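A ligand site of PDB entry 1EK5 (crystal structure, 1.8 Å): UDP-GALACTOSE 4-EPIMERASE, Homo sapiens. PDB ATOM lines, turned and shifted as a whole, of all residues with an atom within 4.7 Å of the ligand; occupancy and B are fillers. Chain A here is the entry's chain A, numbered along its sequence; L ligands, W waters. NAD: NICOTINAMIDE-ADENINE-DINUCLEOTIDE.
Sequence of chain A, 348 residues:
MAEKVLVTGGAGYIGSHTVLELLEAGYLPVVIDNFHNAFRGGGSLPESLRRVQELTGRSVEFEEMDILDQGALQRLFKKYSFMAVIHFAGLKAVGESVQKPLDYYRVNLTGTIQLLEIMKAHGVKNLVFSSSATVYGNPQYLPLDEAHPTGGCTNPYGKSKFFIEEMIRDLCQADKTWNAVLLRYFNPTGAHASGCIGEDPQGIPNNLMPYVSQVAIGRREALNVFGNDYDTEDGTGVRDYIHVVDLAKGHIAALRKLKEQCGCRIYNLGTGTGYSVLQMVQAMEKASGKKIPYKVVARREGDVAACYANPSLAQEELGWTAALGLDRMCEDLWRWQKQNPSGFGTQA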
ATOM      1  N   GLY A   9      24.820  17.472  -9.140  1.00  0.00           N
ATOM      2  CA  GLY A   9      25.033  18.031  -7.812  1.00  0.00           C
ATOM      3  C   GLY A   9      26.521  18.408  -7.596  1.00  0.00           C
ATOM      4  O   GLY A   9      27.076  18.338  -6.485  1.00  0.00           O
ATOM      5  N   ALA A  11      28.012  21.232  -7.644  1.00  0.00           N
ATOM      6  CA  ALA A  11      28.284  22.500  -6.959  1.00  0.00           C
ATOM      7  C   ALA A  11      28.426  22.356  -5.452  1.00  0.00           C
ATOM      8  O   ALA A  11      28.866  23.274  -4.773  1.00  0.00           O
ATOM      9  CB  ALA A  11      27.261  23.559  -7.321  1.00  0.00           C
ATOM     10  N   GLY A  12      28.059  21.160  -4.956  1.00  0.00           N
ATOM     11  CA  GLY A  12      28.072  20.817  -3.572  1.00  0.00           C
ATOM     12  C   GLY A  12      29.446  20.558  -3.038  1.00  0.00           C
ATOM     13  O   GLY A  12      30.437  20.736  -3.734  1.00  0.00           O
ATOM     14  N   TYR A  13      29.445  20.118  -1.793  1.00  0.00           N
ATOM     15  CA  TYR A  13      30.648  19.840  -1.067  1.00  0.00           C
ATOM     16  C   TYR A  13      31.525  18.786  -1.696  1.00  0.00           C
ATOM     17  O   TYR A  13      32.672  19.050  -2.062  1.00  0.00           O
ATOM     18  CB  TYR A  13      30.386  19.585   0.397  1.00  0.00           C
ATOM     19  CG  TYR A  13      31.572  19.234   1.286  1.00  0.00           C
ATOM     20  CD1 TYR A  13      32.770  19.942   1.246  1.00  0.00           C
ATOM     21  CD2 TYR A  13      31.462  18.164   2.177  1.00  0.00           C
ATOM     22  CE1 TYR A  13      33.807  19.593   2.108  1.00  0.00           C
ATOM     23  CE2 TYR A  13      32.494  17.772   3.028  1.00  0.00           C
ATOM     24  CZ  TYR A  13      33.672  18.529   2.972  1.00  0.00           C
ATOM     25  OH  TYR A  13      34.708  18.200   3.810  1.00  0.00           O
ATOM     26  N   ILE A  14      30.977  17.587  -1.798  1.00  0.00           N
ATOM     27  CA  ILE A  14      31.733  16.504  -2.380  1.00  0.00           C
ATOM     28  C   ILE A  14      31.889  16.705  -3.875  1.00  0.00           C
ATOM     29  O   ILE A  14      32.964  16.451  -4.435  1.00  0.00           O
ATOM     30  CB  ILE A  14      31.215  15.101  -2.051  1.00  0.00           C
ATOM     31  CG1 ILE A  14      31.016  14.941  -0.552  1.00  0.00           C
ATOM     32  CG2 ILE A  14      32.251  14.084  -2.524  1.00  0.00           C
ATOM     33  CD1 ILE A  14      30.375  13.629  -0.157  1.00  0.00           C
ATOM     34  N   GLY A  15      30.840  17.181  -4.538  1.00  0.00           N
ATOM     35  CA  GLY A  15      30.875  17.389  -5.963  1.00  0.00           C
ATOM     36  C   GLY A  15      31.947  18.398  -6.421  1.00  0.00           C
ATOM     37  O   GLY A  15      32.700  18.131  -7.348  1.00  0.00           O
ATOM     38  N   ILE A  32      25.755  19.817 -13.347  1.00  0.00           N
ATOM     39  CA  ILE A  32      24.381  20.275 -13.216  1.00  0.00           C
ATOM     40  C   ILE A  32      24.040  20.331 -11.726  1.00  0.00           C
ATOM     41  O   ILE A  32      24.460  19.469 -10.939  1.00  0.00           O
ATOM     42  CB  ILE A  32      23.309  19.481 -13.943  1.00  0.00           C
ATOM     43  CG1 ILE A  32      23.284  18.108 -13.287  1.00  0.00           C
ATOM     44  CG2 ILE A  32      23.661  19.363 -15.412  1.00  0.00           C
ATOM     45  CD1 ILE A  32      22.046  17.350 -13.678  1.00  0.00           C
ATOM     46  N   ASP A  33      23.294  21.358 -11.346  1.00  0.00           N
ATOM     47  CA  ASP A  33      22.883  21.564  -9.970  1.00  0.00           C
ATOM     48  C   ASP A  33      21.657  22.460  -9.982  1.00  0.00           C
ATOM     49  O   ASP A  33      21.516  23.290 -10.886  1.00  0.00           O
ATOM     50  CB  ASP A  33      23.970  22.208  -9.084  1.00  0.00           C
ATOM     51  CG  ASP A  33      23.952  21.818  -7.627  1.00  0.00           C
ATOM     52  OD1 ASP A  33      24.753  21.070  -7.103  1.00  0.00           O
ATOM     53  OD2 ASP A  33      22.992  22.384  -6.926  1.00  0.00           O
ATOM     54  N   ASN A  34      20.793  22.324  -8.972  1.00  0.00           N
ATOM     55  CA  ASN A  34      19.607  23.160  -8.930  1.00  0.00           C
ATOM     56  C   ASN A  34      19.758  24.204  -7.848  1.00  0.00           C
ATOM     57  O   ASN A  34      18.869  24.964  -7.533  1.00  0.00           O
ATOM     58  CB  ASN A  34      18.302  22.348  -8.728  1.00  0.00           C
ATOM     59  CG  ASN A  34      18.209  21.756  -7.334  1.00  0.00           C
ATOM     60  OD1 ASN A  34      19.171  21.799  -6.548  1.00  0.00           O
ATOM     61  ND2 ASN A  34      17.053  21.187  -6.989  1.00  0.00           N
ATOM     62  N   PHE A  35      20.906  24.197  -7.225  1.00  0.00           N
ATOM     63  CA  PHE A  35      21.169  25.180  -6.189  1.00  0.00           C
ATOM     64  C   PHE A  35      20.349  24.933  -4.918  1.00  0.00           C
ATOM     65  O   PHE A  35      20.203  25.820  -4.090  1.00  0.00           O
ATOM     66  CB  PHE A  35      20.983  26.631  -6.685  1.00  0.00           C
ATOM     67  CG  PHE A  35      22.023  27.176  -7.654  1.00  0.00           C
ATOM     68  CD1 PHE A  35      21.743  27.230  -9.015  1.00  0.00           C
ATOM     69  CD2 PHE A  35      23.262  27.667  -7.220  1.00  0.00           C
ATOM     70  CE1 PHE A  35      22.659  27.738  -9.942  1.00  0.00           C
ATOM     71  CE2 PHE A  35      24.190  28.191  -8.122  1.00  0.00           C
ATOM     72  CZ  PHE A  35      23.890  28.223  -9.480  1.00  0.00           C
ATOM     73  N   HIS A  36      19.837  23.738  -4.729  1.00  0.00           N
ATOM     74  CA  HIS A  36      19.075  23.504  -3.519  1.00  0.00           C
ATOM     75  C   HIS A  36      19.954  23.645  -2.298  1.00  0.00           C
ATOM     76  O   HIS A  36      19.539  24.039  -1.215  1.00  0.00           O
ATOM     77  CB  HIS A  36      18.446  22.108  -3.540  1.00  0.00           C
ATOM     78  CG  HIS A  36      18.092  21.699  -2.172  1.00  0.00           C
ATOM     79  ND1 HIS A  36      16.874  22.097  -1.649  1.00  0.00           N
ATOM     80  CD2 HIS A  36      18.766  20.954  -1.258  1.00  0.00           C
ATOM     81  CE1 HIS A  36      16.854  21.607  -0.418  1.00  0.00           C
ATOM     82  NE2 HIS A  36      17.981  20.937  -0.135  1.00  0.00           N
ATOM     83  N   ASN A  37      21.200  23.331  -2.458  1.00  0.00           N
ATOM     84  CA  ASN A  37      22.042  23.440  -1.311  1.00  0.00           C
ATOM     85  C   ASN A  37      23.444  23.937  -1.659  1.00  0.00           C
ATOM     86  O   ASN A  37      24.417  23.529  -1.056  1.00  0.00           O
ATOM     87  CB  ASN A  37      22.175  22.101  -0.610  1.00  0.00           C
ATOM     88  CG  ASN A  37      22.648  22.217   0.827  1.00  0.00           C
ATOM     89  OD1 ASN A  37      22.149  23.037   1.600  1.00  0.00           O
ATOM     90  ND2 ASN A  37      23.625  21.385   1.233  1.00  0.00           N
ATOM     91  N   ALA A  38      23.513  24.855  -2.611  1.00  0.00           N
ATOM     92  CA  ALA A  38      24.778  25.447  -3.005  1.00  0.00           C
ATOM     93  C   ALA A  38      24.596  26.934  -3.251  1.00  0.00           C
ATOM     94  O   ALA A  38      23.572  27.382  -3.711  1.00  0.00           O
ATOM     95  CB  ALA A  38      25.410  24.785  -4.218  1.00  0.00           C
ATOM     96  N   MET A  65      19.958  23.029 -13.305  1.00  0.00           N
ATOM     97  CA  MET A  65      18.790  22.239 -13.626  1.00  0.00           C
ATOM     98  C   MET A  65      18.544  21.251 -12.518  1.00  0.00           C
ATOM     99  O   MET A  65      19.435  21.038 -11.699  1.00  0.00           O
ATOM    100  CB  MET A  65      18.861  21.530 -14.996  1.00  0.00           C
ATOM    101  CG  MET A  65      19.798  20.329 -14.981  1.00  0.00           C
ATOM    102  SD  MET A  65      19.738  19.335 -16.501  1.00  0.00           S
ATOM    103  CE  MET A  65      20.107  20.562 -17.762  1.00  0.00           C
ATOM    104  N   ASP A  66      17.317  20.704 -12.511  1.00  0.00           N
ATOM    105  CA  ASP A  66      16.891  19.735 -11.534  1.00  0.00           C
ATOM    106  C   ASP A  66      16.809  18.387 -12.200  1.00  0.00           C
ATOM    107  O   ASP A  66      16.293  18.287 -13.323  1.00  0.00           O
ATOM    108  CB  ASP A  66      15.495  20.136 -11.008  1.00  0.00           C
ATOM    109  CG  ASP A  66      15.101  19.483  -9.720  1.00  0.00           C
ATOM    110  OD1 ASP A  66      15.294  18.300  -9.470  1.00  0.00           O
ATOM    111  OD2 ASP A  66      14.505  20.282  -8.874  1.00  0.00           O
ATOM    112  N   ILE A  67      17.358  17.363 -11.512  1.00  0.00           N
ATOM    113  CA  ILE A  67      17.341  16.006 -12.052  1.00  0.00           C
ATOM    114  C   ILE A  67      15.900  15.458 -12.134  1.00  0.00           C
ATOM    115  O   ILE A  67      15.638  14.447 -12.772  1.00  0.00           O
ATOM    116  CB  ILE A  67      18.250  15.035 -11.295  1.00  0.00           C
ATOM    117  CG1 ILE A  67      17.852  14.933  -9.832  1.00  0.00           C
ATOM    118  CG2 ILE A  67      19.715  15.420 -11.455  1.00  0.00           C
ATOM    119  CD1 ILE A  67      18.708  13.939  -9.071  1.00  0.00           C
ATOM    120  N   HIS A  87      27.124  10.554  -9.900  1.00  0.00           N
ATOM    121  CA  HIS A  87      25.880  11.031  -9.295  1.00  0.00           C
ATOM    122  C   HIS A  87      25.965  11.401  -7.823  1.00  0.00           C
ATOM    123  O   HIS A  87      26.107  10.550  -6.942  1.00  0.00           O
ATOM    124  CB  HIS A  87      24.843   9.934  -9.606  1.00  0.00           C
ATOM    125  CG  HIS A  87      23.444  10.232  -9.153  1.00  0.00           C
ATOM    126  ND1 HIS A  87      22.864  11.478  -9.368  1.00  0.00           N
ATOM    127  CD2 HIS A  87      22.541   9.453  -8.514  1.00  0.00           C
ATOM    128  CE1 HIS A  87      21.629  11.414  -8.886  1.00  0.00           C
ATOM    129  NE2 HIS A  87      21.418  10.216  -8.350  1.00  0.00           N
ATOM    130  N   PHE A  88      25.953  12.710  -7.607  1.00  0.00           N
ATOM    131  CA  PHE A  88      26.003  13.259  -6.268  1.00  0.00           C
ATOM    132  C   PHE A  88      24.664  13.952  -5.911  1.00  0.00           C
ATOM    133  O   PHE A  88      24.442  14.191  -4.737  1.00  0.00           O
ATOM    134  CB  PHE A  88      27.066  14.385  -6.170  1.00  0.00           C
ATOM    135  CG  PHE A  88      28.513  13.937  -6.268  1.00  0.00           C
ATOM    136  CD1 PHE A  88      29.040  13.171  -5.222  1.00  0.00           C
ATOM    137  CD2 PHE A  88      29.321  14.296  -7.340  1.00  0.00           C
ATOM    138  CE1 PHE A  88      30.357  12.729  -5.245  1.00  0.00           C
ATOM    139  CE2 PHE A  88      30.649  13.868  -7.385  1.00  0.00           C
ATOM    140  CZ  PHE A  88      31.147  13.072  -6.355  1.00  0.00           C
ATOM    141  N   ALA A  89      23.844  14.358  -6.918  1.00  0.00           N
ATOM    142  CA  ALA A  89      22.602  15.105  -6.724  1.00  0.00           C
ATOM    143  C   ALA A  89      21.665  14.421  -5.755  1.00  0.00           C
ATOM    144  O   ALA A  89      21.351  13.267  -5.947  1.00  0.00           O
ATOM    145  CB  ALA A  89      21.937  15.412  -8.068  1.00  0.00           C
ATOM    146  N   GLY A  90      21.211  15.096  -4.697  1.00  0.00           N
ATOM    147  CA  GLY A  90      20.324  14.455  -3.738  1.00  0.00           C
ATOM    148  C   GLY A  90      20.235  15.225  -2.450  1.00  0.00           C
ATOM    149  O   GLY A  90      20.937  16.210  -2.313  1.00  0.00           O
ATOM    150  N   LEU A  91      19.335  14.816  -1.535  1.00  0.00           N
ATOM    151  CA  LEU A  91      19.160  15.429  -0.196  1.00  0.00           C
ATOM    152  C   LEU A  91      19.950  14.546   0.745  1.00  0.00           C
ATOM    153  O   LEU A  91      19.901  13.315   0.565  1.00  0.00           O
ATOM    154  CB  LEU A  91      17.673  15.605   0.237  1.00  0.00           C
ATOM    155  CG  LEU A  91      16.782  16.219  -0.839  1.00  0.00           C
ATOM    156  CD1 LEU A  91      15.339  16.271  -0.344  1.00  0.00           C
ATOM    157  CD2 LEU A  91      17.209  17.638  -1.059  1.00  0.00           C
ATOM    158  N   LYS A  92      20.735  15.100   1.678  1.00  0.00           N
ATOM    159  CA  LYS A  92      21.566  14.228   2.502  1.00  0.00           C
ATOM    160  C   LYS A  92      21.681  14.521   3.986  1.00  0.00           C
ATOM    161  O   LYS A  92      22.569  13.956   4.640  1.00  0.00           O
ATOM    162  CB  LYS A  92      22.990  14.080   1.902  1.00  0.00           C
ATOM    163  CG  LYS A  92      23.574  15.419   1.503  1.00  0.00           C
ATOM    164  CD  LYS A  92      23.758  16.286   2.736  1.00  0.00           C
ATOM    165  CE  LYS A  92      25.156  16.708   3.107  1.00  0.00           C
ATOM    166  NZ  LYS A  92      25.222  18.161   3.126  1.00  0.00           N
ATOM    167  N   VAL A 107      13.135  13.197  -4.075  1.00  0.00           N
ATOM    168  CA  VAL A 107      14.350  13.651  -4.723  1.00  0.00           C
ATOM    169  C   VAL A 107      15.363  12.513  -5.021  1.00  0.00           C
ATOM    170  O   VAL A 107      15.864  12.339  -6.133  1.00  0.00           O
ATOM    171  CB  VAL A 107      14.989  14.818  -3.936  1.00  0.00           C
ATOM    172  CG1 VAL A 107      16.335  15.142  -4.573  1.00  0.00           C
ATOM    173  CG2 VAL A 107      14.112  16.078  -3.920  1.00  0.00           C
ATOM    174  N   SER A 130      27.546   7.888  -5.702  1.00  0.00           N
ATOM    175  CA  SER A 130      28.077   8.305  -4.412  1.00  0.00           C
ATOM    176  C   SER A 130      27.087   7.821  -3.345  1.00  0.00           C
ATOM    177  O   SER A 130      26.078   8.455  -3.114  1.00  0.00           O
ATOM    178  CB  SER A 130      28.395   9.800  -4.404  1.00  0.00           C
ATOM    179  OG  SER A 130      29.397  10.063  -3.426  1.00  0.00           O
ATOM    180  N   SER A 131      27.415   6.682  -2.720  1.00  0.00           N
ATOM    181  CA  SER A 131      26.607   6.030  -1.738  1.00  0.00           C
ATOM    182  C   SER A 131      26.885   6.418  -0.285  1.00  0.00           C
ATOM    183  O   SER A 131      27.430   7.475   0.008  1.00  0.00           O
ATOM    184  CB  SER A 131      26.621   4.530  -1.954  1.00  0.00           C
ATOM    185  OG  SER A 131      25.541   3.953  -1.242  1.00  0.00           O
ATOM    186  N   SER A 132      26.515   5.570   0.649  1.00  0.00           N
ATOM    187  CA  SER A 132      26.747   5.869   2.034  1.00  0.00           C
ATOM    188  C   SER A 132      26.977   4.599   2.818  1.00  0.00           C
ATOM    189  O   SER A 132      26.257   3.629   2.689  1.00  0.00           O
ATOM    190  CB  SER A 132      25.625   6.712   2.663  1.00  0.00           C
ATOM    191  OG  SER A 132      25.799   6.693   4.084  1.00  0.00           O
ATOM    192  N   TYR A 157      17.008   8.817   5.146  1.00  0.00           N
ATOM    193  CA  TYR A 157      18.160   9.071   4.262  1.00  0.00           C
ATOM    194  C   TYR A 157      18.865   7.765   3.843  1.00  0.00           C
ATOM    195  O   TYR A 157      19.060   7.434   2.679  1.00  0.00           O
ATOM    196  CB  TYR A 157      19.140  10.080   4.923  1.00  0.00           C
ATOM    197  CG  TYR A 157      20.448  10.129   4.143  1.00  0.00           C
ATOM    198  CD1 TYR A 157      21.579   9.457   4.590  1.00  0.00           C
ATOM    199  CD2 TYR A 157      20.530  10.834   2.948  1.00  0.00           C
ATOM    200  CE1 TYR A 157      22.788   9.478   3.878  1.00  0.00           C
ATOM    201  CE2 TYR A 157      21.731  10.854   2.224  1.00  0.00           C
ATOM    202  CZ  TYR A 157      22.872  10.190   2.690  1.00  0.00           C
ATOM    203  OH  TYR A 157      24.103  10.183   1.999  1.00  0.00           O
ATOM    204  N   LYS A 161      19.301   5.577   0.306  1.00  0.00           N
ATOM    205  CA  LYS A 161      20.611   5.230  -0.258  1.00  0.00           C
ATOM    206  C   LYS A 161      20.635   3.766  -0.671  1.00  0.00           C
ATOM    207  O   LYS A 161      20.961   3.418  -1.799  1.00  0.00           O
ATOM    208  CB  LYS A 161      21.764   5.566   0.688  1.00  0.00           C
ATOM    209  CG  LYS A 161      21.965   7.051   0.930  1.00  0.00           C
ATOM    210  CD  LYS A 161      21.998   7.952  -0.312  1.00  0.00           C
ATOM    211  CE  LYS A 161      23.296   7.879  -1.137  1.00  0.00           C
ATOM    212  NZ  LYS A 161      23.594   9.054  -1.987  1.00  0.00           N
ATOM    213  N   TYR A 185      30.877   5.308   1.869  1.00  0.00           N
ATOM    214  CA  TYR A 185      31.778   5.963   2.786  1.00  0.00           C
ATOM    215  C   TYR A 185      30.947   6.574   3.896  1.00  0.00           C
ATOM    216  O   TYR A 185      29.712   6.617   3.785  1.00  0.00           O
ATOM    217  CB  TYR A 185      32.604   7.056   2.068  1.00  0.00           C
ATOM    218  CG  TYR A 185      31.760   8.013   1.263  1.00  0.00           C
ATOM    219  CD1 TYR A 185      31.367   7.712  -0.040  1.00  0.00           C
ATOM    220  CD2 TYR A 185      31.350   9.232   1.821  1.00  0.00           C
ATOM    221  CE1 TYR A 185      30.595   8.595  -0.791  1.00  0.00           C
ATOM    222  CE2 TYR A 185      30.575  10.130   1.086  1.00  0.00           C
ATOM    223  CZ  TYR A 185      30.186   9.793  -0.210  1.00  0.00           C
ATOM    224  OH  TYR A 185      29.428  10.663  -0.935  1.00  0.00           O
ATOM    225  N   PHE A 186      31.654   7.016   4.937  1.00  0.00           N
ATOM    226  CA  PHE A 186      31.035   7.621   6.131  1.00  0.00           C
ATOM    227  C   PHE A 186      31.033   9.129   6.150  1.00  0.00           C
ATOM    228  O   PHE A 186      30.238   9.793   5.460  1.00  0.00           O
ATOM    229  CB  PHE A 186      31.552   7.041   7.466  1.00  0.00           C
ATOM    230  CG  PHE A 186      31.011   5.659   7.814  1.00  0.00           C
ATOM    231  CD1 PHE A 186      29.677   5.526   8.214  1.00  0.00           C
ATOM    232  CD2 PHE A 186      31.784   4.501   7.728  1.00  0.00           C
ATOM    233  CE1 PHE A 186      29.153   4.271   8.531  1.00  0.00           C
ATOM    234  CE2 PHE A 186      31.274   3.239   8.030  1.00  0.00           C
ATOM    235  CZ  PHE A 186      29.932   3.120   8.434  1.00  0.00           C
ATOM    236  N   PRO A 188      32.590  12.644   5.360  1.00  0.00           N
ATOM    237  CA  PRO A 188      33.555  13.464   4.624  1.00  0.00           C
ATOM    238  C   PRO A 188      33.915  14.655   5.458  1.00  0.00           C
ATOM    239  O   PRO A 188      33.036  15.269   6.076  1.00  0.00           O
ATOM    240  CB  PRO A 188      32.833  14.020   3.370  1.00  0.00           C
ATOM    241  CG  PRO A 188      31.343  13.829   3.638  1.00  0.00           C
ATOM    242  CD  PRO A 188      31.240  12.782   4.763  1.00  0.00           C
ATOM    243  N   ASN A 206      25.862  16.459   9.725  1.00  0.00           N
ATOM    244  CA  ASN A 206      25.745  15.015   9.804  1.00  0.00           C
ATOM    245  C   ASN A 206      26.759  14.456  10.750  1.00  0.00           C
ATOM    246  O   ASN A 206      26.692  13.302  11.195  1.00  0.00           O
ATOM    247  CB  ASN A 206      25.948  14.407   8.410  1.00  0.00           C
ATOM    248  CG  ASN A 206      24.664  14.426   7.610  1.00  0.00           C
ATOM    249  OD1 ASN A 206      23.584  14.539   8.179  1.00  0.00           O
ATOM    250  ND2 ASN A 206      24.751  14.327   6.283  1.00  0.00           N
HETATM  251  PA  NAD L   1      25.804  18.706  -0.897  1.00  0.00           P
HETATM  252  O1A NAD L   1      24.446  19.147  -0.472  1.00  0.00           O
HETATM  253  O2A NAD L   1      26.860  19.719  -0.593  1.00  0.00           O
HETATM  254  O5B NAD L   1      25.698  18.552  -2.472  1.00  0.00           O
HETATM  255  C5B NAD L   1      24.565  17.963  -3.139  1.00  0.00           C
HETATM  256  C4B NAD L   1      24.260  18.960  -4.229  1.00  0.00           C
HETATM  257  O4B NAD L   1      23.145  18.502  -5.013  1.00  0.00           O
HETATM  258  C3B NAD L   1      23.926  20.367  -3.806  1.00  0.00           C
HETATM  259  O3B NAD L   1      24.689  21.244  -4.608  1.00  0.00           O
HETATM  260  C2B NAD L   1      22.430  20.462  -4.096  1.00  0.00           C
HETATM  261  O2B NAD L   1      22.075  21.784  -4.485  1.00  0.00           O
HETATM  262  C1B NAD L   1      22.358  19.576  -5.329  1.00  0.00           C
HETATM  263  N9A NAD L   1      21.041  18.999  -5.521  1.00  0.00           N
HETATM  264  C8A NAD L   1      20.155  18.557  -4.557  1.00  0.00           C
HETATM  265  N7A NAD L   1      18.983  18.184  -5.101  1.00  0.00           N
HETATM  266  C5A NAD L   1      19.158  18.397  -6.471  1.00  0.00           C
HETATM  267  C6A NAD L   1      18.319  18.219  -7.569  1.00  0.00           C
HETATM  268  N6A NAD L   1      17.063  17.767  -7.464  1.00  0.00           N
HETATM  269  N1A NAD L   1      18.817  18.480  -8.812  1.00  0.00           N
HETATM  270  C2A NAD L   1      20.090  18.961  -8.927  1.00  0.00           C
HETATM  271  N3A NAD L   1      20.933  19.162  -7.976  1.00  0.00           N
HETATM  272  C4A NAD L   1      20.436  18.837  -6.754  1.00  0.00           C
HETATM  273  O3  NAD L   1      26.136  17.402  -0.156  1.00  0.00           O
HETATM  274  PN  NAD L   1      27.293  16.298  -0.369  1.00  0.00           P
HETATM  275  O1N NAD L   1      27.617  15.721   0.962  1.00  0.00           O
HETATM  276  O2N NAD L   1      28.437  17.109  -0.887  1.00  0.00           O
HETATM  277  O5D NAD L   1      27.177  15.067  -1.342  1.00  0.00           O
HETATM  278  C5D NAD L   1      26.040  14.786  -2.100  1.00  0.00           C
HETATM  279  C4D NAD L   1      26.061  13.295  -2.280  1.00  0.00           C
HETATM  280  O4D NAD L   1      27.004  12.742  -1.321  1.00  0.00           O
HETATM  281  C3D NAD L   1      24.712  12.626  -2.030  1.00  0.00           C
HETATM  282  O3D NAD L   1      24.530  11.557  -2.953  1.00  0.00           O
HETATM  283  C2D NAD L   1      24.938  12.156  -0.582  1.00  0.00           C
HETATM  284  O2D NAD L   1      24.014  11.119  -0.230  1.00  0.00           O
HETATM  285  C1D NAD L   1      26.381  11.666  -0.644  1.00  0.00           C
HETATM  286  N1N NAD L   1      26.955  11.506   0.699  1.00  0.00           N
HETATM  287  C2N NAD L   1      27.141  12.654   1.457  1.00  0.00           C
HETATM  288  C3N NAD L   1      27.480  12.423   2.756  1.00  0.00           C
HETATM  289  C7N NAD L   1      27.636  13.598   3.695  1.00  0.00           C
HETATM  290  O7N NAD L   1      27.931  13.226   4.841  1.00  0.00           O
HETATM  291  N7N NAD L   1      27.524  14.914   3.342  1.00  0.00           N
HETATM  292  C4N NAD L   1      27.745  11.167   3.323  1.00  0.00           C
HETATM  293  C5N NAD L   1      27.583  10.123   2.460  1.00  0.00           C
HETATM  294  C6N NAD L   1      27.232  10.212   1.158  1.00  0.00           C
HETATM  295  O   HOH W   1      28.707  13.220   7.464  1.00  0.00           O
HETATM  296  O   HOH W   2      21.591  11.931  -1.424  1.00  0.00           O
HETATM  297  O   HOH W   3      16.369  19.276  -4.574  1.00  0.00           O
HETATM  298  O   HOH W   4      28.270  17.623  -4.002  1.00  0.00           O
HETATM  299  O   HOH W   5      23.118  11.139  -5.288  1.00  0.00           O
HETATM  300  O   HOH W   6      28.366  16.790   5.066  1.00  0.00           O
HETATM  301  O   HOH W   7      21.565  18.613  -0.956  1.00  0.00           O
HETATM  302  O   HOH W   8      27.521   8.340   5.084  1.00  0.00           O
HETATM  303  O   HOH W   9      26.972  22.410  -0.202  1.00  0.00           O
HETATM  304  O   HOH W  10      24.711  12.028   4.011  1.00  0.00           O
HETATM  305  O   HOH W  11      27.162  19.957   2.269  1.00  0.00           O
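O2B of the ligand is in hydrogen-bond range of N of Asn 37 (2.7 Å). O2A of the ligand is in hydrogen-bond range of N of Tyr 13, at 2.9 Å. An oxygen (O3B) of the ligand sits at hydrogen-bond distance from the backbone NH (N) of Gly 12 (3.4 Å). O1A of the ligand is in hydrogen-bond range of ND2 of Asn 37, 2.9 Å away. N1A of the ligand sits at hydrogen-bond distance from N of Ile 67 (3.3 Å). The backbone carbonyl oxygen of Phe 88 sits close to an oxygen (O3D) of the ligand (3.2 Å). An oxygen (O3B) of the ligand sits at hydrogen-bond distance from the side-chain carboxylate (OD1) of Asp 33, 2.5 Å away. NZ of Lys 92 lies within salt-bridge range of O1A of the ligand, at 3.8 Å. OD1 of Asp 66 lies within hydrogen-bond range of N6A of the ligand, 2.7 Å away. The backbone NH (N) of Ile 14 sits at hydrogen-bond distance from an oxygen (O2N) of the ligand (2.7 Å). An oxygen (O3D) of the ligand is in hydrogen-bond range of the backbone carbonyl oxygen (O) of Ser 130, 3.5 Å away. O4D of the ligand sits close to OH of Tyr 185, 3.2 Å away. O2B of the ligand sits at hydrogen-bond distance from N of His 36, at 3.0 Å. The side-chain amide nitrogen (ND2) of Asn 34 sits close to a nitrogen (N6A) of the ligand (3.5 Å). An oxygen (O2D) of the ligand is in hydrogen-bond range of the side-chain hydroxyl of Tyr 157 (2.4 Å). NZ of Lys 161 lies within hydrogen-bond range of O2D of the ligand, 2.7 Å away. The backbone NH (N) of Asn 34 lies within hydrogen-bond range of a nitrogen (N3A) of the ligand (3.3 Å).
Residues that only touch the ligand: Ser 131 (3.0 Å), Pro 188 (3.3 Å), Gly 90 (3.3 Å), Gly 9 (3.4 Å), Met 65 (3.5 Å), Phe 186 (3.6 Å), Phe 35 (3.6 Å), Ala 38 (3.6 Å), Asn 206 (3.7 Å), Ala 89 (3.8 Å), Ser 132 (3.9 Å), Val 107 (3.97 Å) and Ala 11 (3.99 Å). Hydrophobic or aromatic side chains that line the ligand: Tyr 13, Ile 14, His 36, Ala 38, Ile 67, Ala 89, Val 107, Tyr 157, Tyr 185 and Pro 188. Of the 32 residues printed, 28 come within 4 Å of the ligand. The nearest printed residue that does not touch the ligand is Gly 15 (4.4 Å).
The side-chain carboxylate of Asp 33 lies within hydrogen-bond range of the backbone NH of Phe 35, at 2.8 Å. The backbone carbonyl oxygen (O) of Asp 33 lies within hydrogen-bond range of the backbone NH (N) of Met 65. The backbone carbonyl oxygen (O) of Ile 32 sits at hydrogen-bond distance from the backbone NH (N) of Gly 9 (2.7 Å). The backbone carbonyl oxygen (O) of Met 65 is in hydrogen-bond range of the backbone NH (N) of Asn 34, at 3.3 Å. The side-chain amide nitrogen of Asn 34 sits at hydrogen-bond distance from the side-chain carboxylate of Asp 66 (3.3 Å). OH of Tyr 185 lies within hydrogen-bond range of OG of Ser 130. The side-chain carboxylate of Asp 33 is in hydrogen-bond range of the backbone NH of Ala 11 (3.3 Å). The backbone carbonyl oxygen of Ser 130 sits at hydrogen-bond distance from the side-chain amino group of Lys 161.
Water W2 bridges O2D of the ligand (2.8 Å) and O of Leu 91 (3.0 Å). Water W3 lies within hydrogen-bond range of a nitrogen (N7A) of the ligand (2.9 Å) and the side-chain amide nitrogen (ND2) of Asn 34 (3.2 Å). Water W11 lies within hydrogen-bond range of NZ of Lys 92 (2.8 Å) and O2A of the ligand (2.9 Å). Water W7 lies within hydrogen-bond range of O of Gly 90 (2.8 Å) and O1A of the ligand (3.0 Å). Water W10 lies within hydrogen-bond range of the side-chain hydroxyl of Tyr 157 (2.8 Å), the backbone carbonyl oxygen of Lys 92 (2.9 Å) and the side-chain amide nitrogen of Asn 206 (3.2 Å). Water W8 lies within hydrogen-bond range of OG of Ser 132, O of Tyr 185 and O of Phe 186.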
